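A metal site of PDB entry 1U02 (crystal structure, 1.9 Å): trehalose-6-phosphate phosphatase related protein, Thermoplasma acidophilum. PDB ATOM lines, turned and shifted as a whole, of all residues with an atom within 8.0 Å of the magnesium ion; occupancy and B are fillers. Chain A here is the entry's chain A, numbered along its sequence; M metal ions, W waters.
The side-chain hydroxyl (OG1) of Thr 11 lies within hydrogen-bond range of the backbone NH (N) of Asp 179.
The side-chain carboxylate of Asp 7 sits close to the side-chain hydroxyl of Thr 11 (2.7 Å).
N of Asp 179 is in hydrogen-bond range of OD2 of Asp 183 (3.0 Å).
The side-chain carboxylate of Asp 7 lies within salt-bridge range of the side-chain amino group of Lys 161 (2.9 Å).
O of Ala 177 sits at hydrogen-bond distance from N of Asp 7, at 3.0 Å.
Water W1 bridges the side-chain carboxylate (OD2) of Asp 179 and the side-chain carboxylate (OD2) of Asp 180.
Within 4 Å of the magnesium ion: Asp 7, Asp 9 and Asp 179.
Along chain A the residues within 4 Å of the magnesium ion span positions 7 to 179.
The magnesium ion is bound by OD1 of Asp 179 (2.0 Å).
The magnesium ion is bound by water W1, at 2.0 Å.
O of Asp 9 is bound to the magnesium ion, 2.1 Å away.
The magnesium ion is bound by OD2 of Asp 7.
Water W3 binds the magnesium ion (2.1 Å).
The magnesium ion is bound by water W2, 2.1 Å away.
The magnesium ion has six donor atoms within binding distance.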
ATOM      1  N   LEU A   6      -5.744  21.830  26.898  1.00  0.00           N
ATOM      2  CA  LEU A   6      -6.527  22.745  26.071  1.00  0.00           C
ATOM      3  C   LEU A   6      -6.963  24.007  26.785  1.00  0.00           C
ATOM      4  O   LEU A   6      -7.553  23.938  27.864  1.00  0.00           O
ATOM      5  CB  LEU A   6      -7.788  22.033  25.571  1.00  0.00           C
ATOM      6  CG  LEU A   6      -7.611  20.686  24.857  1.00  0.00           C
ATOM      7  CD1 LEU A   6      -8.955  19.963  24.761  1.00  0.00           C
ATOM      8  CD2 LEU A   6      -6.999  20.915  23.492  1.00  0.00           C
ATOM      9  N   ASP A   7      -6.673  25.154  26.179  1.00  0.00           N
ATOM     10  CA  ASP A   7      -7.104  26.436  26.728  1.00  0.00           C
ATOM     11  C   ASP A   7      -8.607  26.430  26.474  1.00  0.00           C
ATOM     12  O   ASP A   7      -9.091  25.695  25.613  1.00  0.00           O
ATOM     13  CB  ASP A   7      -6.441  27.592  25.956  1.00  0.00           C
ATOM     14  CG  ASP A   7      -7.045  28.948  26.296  1.00  0.00           C
ATOM     15  OD1 ASP A   7      -7.089  29.312  27.489  1.00  0.00           O
ATOM     16  OD2 ASP A   7      -7.476  29.646  25.360  1.00  0.00           O
ATOM     17  N   TYR A   8      -9.361  27.243  27.207  1.00  0.00           N
ATOM     18  CA  TYR A   8     -10.806  27.284  27.033  1.00  0.00           C
ATOM     19  C   TYR A   8     -11.281  28.458  26.167  1.00  0.00           C
ATOM     20  O   TYR A   8     -11.685  28.263  25.009  1.00  0.00           O
ATOM     21  CB  TYR A   8     -11.506  27.353  28.405  1.00  0.00           C
ATOM     22  CG  TYR A   8     -12.996  27.123  28.360  1.00  0.00           C
ATOM     23  CD1 TYR A   8     -13.521  25.861  28.032  1.00  0.00           C
ATOM     24  CD2 TYR A   8     -13.893  28.153  28.607  1.00  0.00           C
ATOM     25  CE1 TYR A   8     -14.896  25.648  27.965  1.00  0.00           C
ATOM     26  CE2 TYR A   8     -15.288  27.954  28.538  1.00  0.00           C
ATOM     27  CZ  TYR A   8     -15.768  26.694  28.218  1.00  0.00           C
ATOM     28  OH  TYR A   8     -17.127  26.480  28.136  1.00  0.00           O
ATOM     29  N   ASP A   9     -11.241  29.676  26.713  1.00  0.00           N
ATOM     30  CA  ASP A   9     -11.685  30.846  25.967  1.00  0.00           C
ATOM     31  C   ASP A   9     -10.866  31.139  24.722  1.00  0.00           C
ATOM     32  O   ASP A   9      -9.637  31.242  24.782  1.00  0.00           O
ATOM     33  CB  ASP A   9     -11.702  32.067  26.878  1.00  0.00           C
ATOM     34  CG  ASP A   9     -12.643  31.887  28.052  1.00  0.00           C
ATOM     35  OD1 ASP A   9     -13.860  31.761  27.809  1.00  0.00           O
ATOM     36  OD2 ASP A   9     -12.162  31.847  29.188  1.00  0.00           O
ATOM     37  N   GLY A  10     -11.557  31.262  23.598  1.00  0.00           N
ATOM     38  CA  GLY A  10     -10.891  31.536  22.335  1.00  0.00           C
ATOM     39  C   GLY A  10     -10.269  30.304  21.718  1.00  0.00           C
ATOM     40  O   GLY A  10      -9.724  30.382  20.605  1.00  0.00           O
ATOM     41  N   THR A  11     -10.322  29.183  22.414  1.00  0.00           N
ATOM     42  CA  THR A  11      -9.751  27.939  21.929  1.00  0.00           C
ATOM     43  C   THR A  11     -10.829  26.878  21.691  1.00  0.00           C
ATOM     44  O   THR A  11     -10.927  26.310  20.606  1.00  0.00           O
ATOM     45  CB  THR A  11      -8.681  27.416  22.903  1.00  0.00           C
ATOM     46  OG1 THR A  11      -7.619  28.386  22.992  1.00  0.00           O
ATOM     47  CG2 THR A  11      -8.100  26.095  22.426  1.00  0.00           C
ATOM     48  N   LEU A  12     -11.641  26.610  22.711  1.00  0.00           N
ATOM     49  CA  LEU A  12     -12.724  25.642  22.601  1.00  0.00           C
ATOM     50  C   LEU A  12     -14.063  26.364  22.403  1.00  0.00           C
ATOM     51  O   LEU A  12     -15.008  25.800  21.859  1.00  0.00           O
ATOM     52  CB  LEU A  12     -12.791  24.748  23.847  1.00  0.00           C
ATOM     53  CG  LEU A  12     -11.534  23.926  24.134  1.00  0.00           C
ATOM     54  CD1 LEU A  12     -11.755  23.054  25.370  1.00  0.00           C
ATOM     55  CD2 LEU A  12     -11.201  23.057  22.924  1.00  0.00           C
ATOM     56  N   VAL A  13     -14.124  27.603  22.872  1.00  0.00           N
ATOM     57  CA  VAL A  13     -15.321  28.422  22.730  1.00  0.00           C
ATOM     58  C   VAL A  13     -14.836  29.779  22.222  1.00  0.00           C
ATOM     59  O   VAL A  13     -13.672  30.121  22.389  1.00  0.00           O
ATOM     60  CB  VAL A  13     -16.061  28.623  24.084  1.00  0.00           C
ATOM     61  CG1 VAL A  13     -16.570  27.284  24.597  1.00  0.00           C
ATOM     62  CG2 VAL A  13     -15.127  29.263  25.104  1.00  0.00           C
ATOM     63  N   ILE A  15     -14.454  33.958  21.886  1.00  0.00           N
ATOM     64  CA  ILE A  15     -14.312  35.068  22.816  1.00  0.00           C
ATOM     65  C   ILE A  15     -15.570  35.874  22.569  1.00  0.00           C
ATOM     66  O   ILE A  15     -15.900  36.179  21.423  1.00  0.00           O
ATOM     67  CB  ILE A  15     -13.085  35.926  22.478  1.00  0.00           C
ATOM     68  CG1 ILE A  15     -11.811  35.096  22.625  1.00  0.00           C
ATOM     69  CG2 ILE A  15     -13.029  37.140  23.402  1.00  0.00           C
ATOM     70  CD1 ILE A  15     -11.565  34.635  24.051  1.00  0.00           C
ATOM     71  N   VAL A  44      -6.762  24.116  30.523  1.00  0.00           N
ATOM     72  CA  VAL A  44      -5.816  25.064  31.131  1.00  0.00           C
ATOM     73  C   VAL A  44      -6.385  26.439  30.857  1.00  0.00           C
ATOM     74  O   VAL A  44      -6.515  26.850  29.709  1.00  0.00           O
ATOM     75  CB  VAL A  44      -4.414  24.928  30.510  1.00  0.00           C
ATOM     76  CG1 VAL A  44      -3.456  25.880  31.203  1.00  0.00           C
ATOM     77  CG2 VAL A  44      -3.929  23.494  30.639  1.00  0.00           C
ATOM     78  N   THR A  45      -6.698  27.177  31.924  1.00  0.00           N
ATOM     79  CA  THR A  45      -7.347  28.464  31.759  1.00  0.00           C
ATOM     80  C   THR A  45      -7.014  29.468  32.849  1.00  0.00           C
ATOM     81  O   THR A  45      -6.391  29.134  33.852  1.00  0.00           O
ATOM     82  CB  THR A  45      -8.872  28.209  31.764  1.00  0.00           C
ATOM     83  OG1 THR A  45      -9.589  29.441  31.713  1.00  0.00           O
ATOM     84  CG2 THR A  45      -9.249  27.441  33.031  1.00  0.00           C
ATOM     85  N   GLY A  46      -7.456  30.707  32.645  1.00  0.00           N
ATOM     86  CA  GLY A  46      -7.252  31.746  33.641  1.00  0.00           C
ATOM     87  C   GLY A  46      -8.511  31.789  34.486  1.00  0.00           C
ATOM     88  O   GLY A  46      -8.568  32.477  35.516  1.00  0.00           O
ATOM     89  N   HIS A  66      -4.378  30.300  35.547  1.00  0.00           N
ATOM     90  CA  HIS A  66      -3.063  30.254  34.914  1.00  0.00           C
ATOM     91  C   HIS A  66      -2.060  29.435  35.729  1.00  0.00           C
ATOM     92  O   HIS A  66      -0.845  29.604  35.586  1.00  0.00           O
ATOM     93  CB  HIS A  66      -2.535  31.678  34.691  1.00  0.00           C
ATOM     94  CG  HIS A  66      -3.258  32.437  33.623  1.00  0.00           C
ATOM     95  ND1 HIS A  66      -3.015  32.243  32.279  1.00  0.00           N
ATOM     96  CD2 HIS A  66      -4.235  33.374  33.704  1.00  0.00           C
ATOM     97  CE1 HIS A  66      -3.807  33.024  31.575  1.00  0.00           C
ATOM     98  NE2 HIS A  66      -4.566  33.722  32.415  1.00  0.00           N
ATOM     99  N   LYS A 161       1.000  29.673  32.861  1.00  0.00           N
ATOM    100  CA  LYS A 161       0.426  28.485  32.219  1.00  0.00           C
ATOM    101  C   LYS A 161       1.512  27.483  31.819  1.00  0.00           C
ATOM    102  O   LYS A 161       1.388  26.283  32.082  1.00  0.00           O
ATOM    103  CB  LYS A 161      -0.338  28.848  30.944  1.00  0.00           C
ATOM    104  CG  LYS A 161      -1.811  29.167  31.112  1.00  0.00           C
ATOM    105  CD  LYS A 161      -2.422  29.438  29.743  1.00  0.00           C
ATOM    106  CE  LYS A 161      -3.907  29.753  29.825  1.00  0.00           C
ATOM    107  NZ  LYS A 161      -4.449  30.134  28.485  1.00  0.00           N
ATOM    108  N   ALA A 177      -2.832  23.378  23.153  1.00  0.00           N
ATOM    109  CA  ALA A 177      -3.545  24.314  22.282  1.00  0.00           C
ATOM    110  C   ALA A 177      -3.977  25.584  23.008  1.00  0.00           C
ATOM    111  O   ALA A 177      -4.469  25.528  24.138  1.00  0.00           O
ATOM    112  CB  ALA A 177      -4.756  23.624  21.671  1.00  0.00           C
ATOM    113  N   GLY A 178      -3.802  26.723  22.351  1.00  0.00           N
ATOM    114  CA  GLY A 178      -4.168  27.999  22.944  1.00  0.00           C
ATOM    115  C   GLY A 178      -4.299  29.080  21.888  1.00  0.00           C
ATOM    116  O   GLY A 178      -3.882  28.870  20.745  1.00  0.00           O
ATOM    117  N   ASP A 179      -4.845  30.232  22.256  1.00  0.00           N
ATOM    118  CA  ASP A 179      -5.066  31.318  21.307  1.00  0.00           C
ATOM    119  C   ASP A 179      -4.371  32.671  21.545  1.00  0.00           C
ATOM    120  O   ASP A 179      -4.364  33.504  20.638  1.00  0.00           O
ATOM    121  CB  ASP A 179      -6.559  31.592  21.191  1.00  0.00           C
ATOM    122  CG  ASP A 179      -7.144  32.158  22.469  1.00  0.00           C
ATOM    123  OD1 ASP A 179      -7.002  31.512  23.519  1.00  0.00           O
ATOM    124  OD2 ASP A 179      -7.731  33.255  22.421  1.00  0.00           O
ATOM    125  N   ASP A 180      -3.835  32.915  22.724  1.00  0.00           N
ATOM    126  CA  ASP A 180      -3.178  34.202  22.943  1.00  0.00           C
ATOM    127  C   ASP A 180      -1.757  34.123  23.489  1.00  0.00           C
ATOM    128  O   ASP A 180      -1.186  33.038  23.572  1.00  0.00           O
ATOM    129  CB  ASP A 180      -4.024  35.105  23.869  1.00  0.00           C
ATOM    130  CG  ASP A 180      -4.154  34.542  25.272  1.00  0.00           C
ATOM    131  OD1 ASP A 180      -3.275  33.760  25.682  1.00  0.00           O
ATOM    132  OD2 ASP A 180      -5.123  34.920  25.963  1.00  0.00           O
ATOM    133  N   ALA A 181      -1.208  35.270  23.857  1.00  0.00           N
ATOM    134  CA  ALA A 181       0.162  35.347  24.371  1.00  0.00           C
ATOM    135  C   ALA A 181       0.493  34.395  25.510  1.00  0.00           C
ATOM    136  O   ALA A 181       1.589  33.825  25.543  1.00  0.00           O
ATOM    137  CB  ALA A 181       0.476  36.781  24.786  1.00  0.00           C
ATOM    138  N   THR A 182      -0.426  34.217  26.450  1.00  0.00           N
ATOM    139  CA  THR A 182      -0.178  33.328  27.574  1.00  0.00           C
ATOM    140  C   THR A 182       0.002  31.895  27.100  1.00  0.00           C
ATOM    141  O   THR A 182       0.696  31.089  27.732  1.00  0.00           O
ATOM    142  CB  THR A 182      -1.328  33.369  28.610  1.00  0.00           C
ATOM    143  OG1 THR A 182      -2.522  32.816  28.028  1.00  0.00           O
ATOM    144  CG2 THR A 182      -1.598  34.814  29.027  1.00  0.00           C
ATOM    145  N   ASP A 183      -0.614  31.566  25.970  1.00  0.00           N
ATOM    146  CA  ASP A 183      -0.508  30.228  25.417  1.00  0.00           C
ATOM    147  C   ASP A 183       0.771  30.165  24.588  1.00  0.00           C
ATOM    148  O   ASP A 183       1.455  29.141  24.552  1.00  0.00           O
ATOM    149  CB  ASP A 183      -1.733  29.917  24.565  1.00  0.00           C
ATOM    150  CG  ASP A 183      -3.017  30.065  25.351  1.00  0.00           C
ATOM    151  OD1 ASP A 183      -3.223  29.268  26.292  1.00  0.00           O
ATOM    152  OD2 ASP A 183      -3.810  30.968  25.020  1.00  0.00           O
ATOM    153  N   VAL A 198      -4.465  28.793  17.917  1.00  0.00           N
ATOM    154  CA  VAL A 198      -5.799  29.051  17.396  1.00  0.00           C
ATOM    155  C   VAL A 198      -5.914  30.540  17.142  1.00  0.00           C
ATOM    156  O   VAL A 198      -5.599  31.351  18.014  1.00  0.00           O
ATOM    157  CB  VAL A 198      -6.902  28.654  18.407  1.00  0.00           C
ATOM    158  CG1 VAL A 198      -8.271  28.941  17.814  1.00  0.00           C
ATOM    159  CG2 VAL A 198      -6.770  27.183  18.789  1.00  0.00           C
HETATM  160 MG    MG M   1      -7.732  31.715  25.397  1.00  0.00          MG
HETATM  161  O   HOH W   1      -8.104  33.701  25.096  1.00  0.00           O
HETATM  162  O   HOH W   2      -5.829  31.987  26.275  1.00  0.00           O
HETATM  163  O   HOH W   3      -8.423  31.838  27.366  1.00  0.00           O
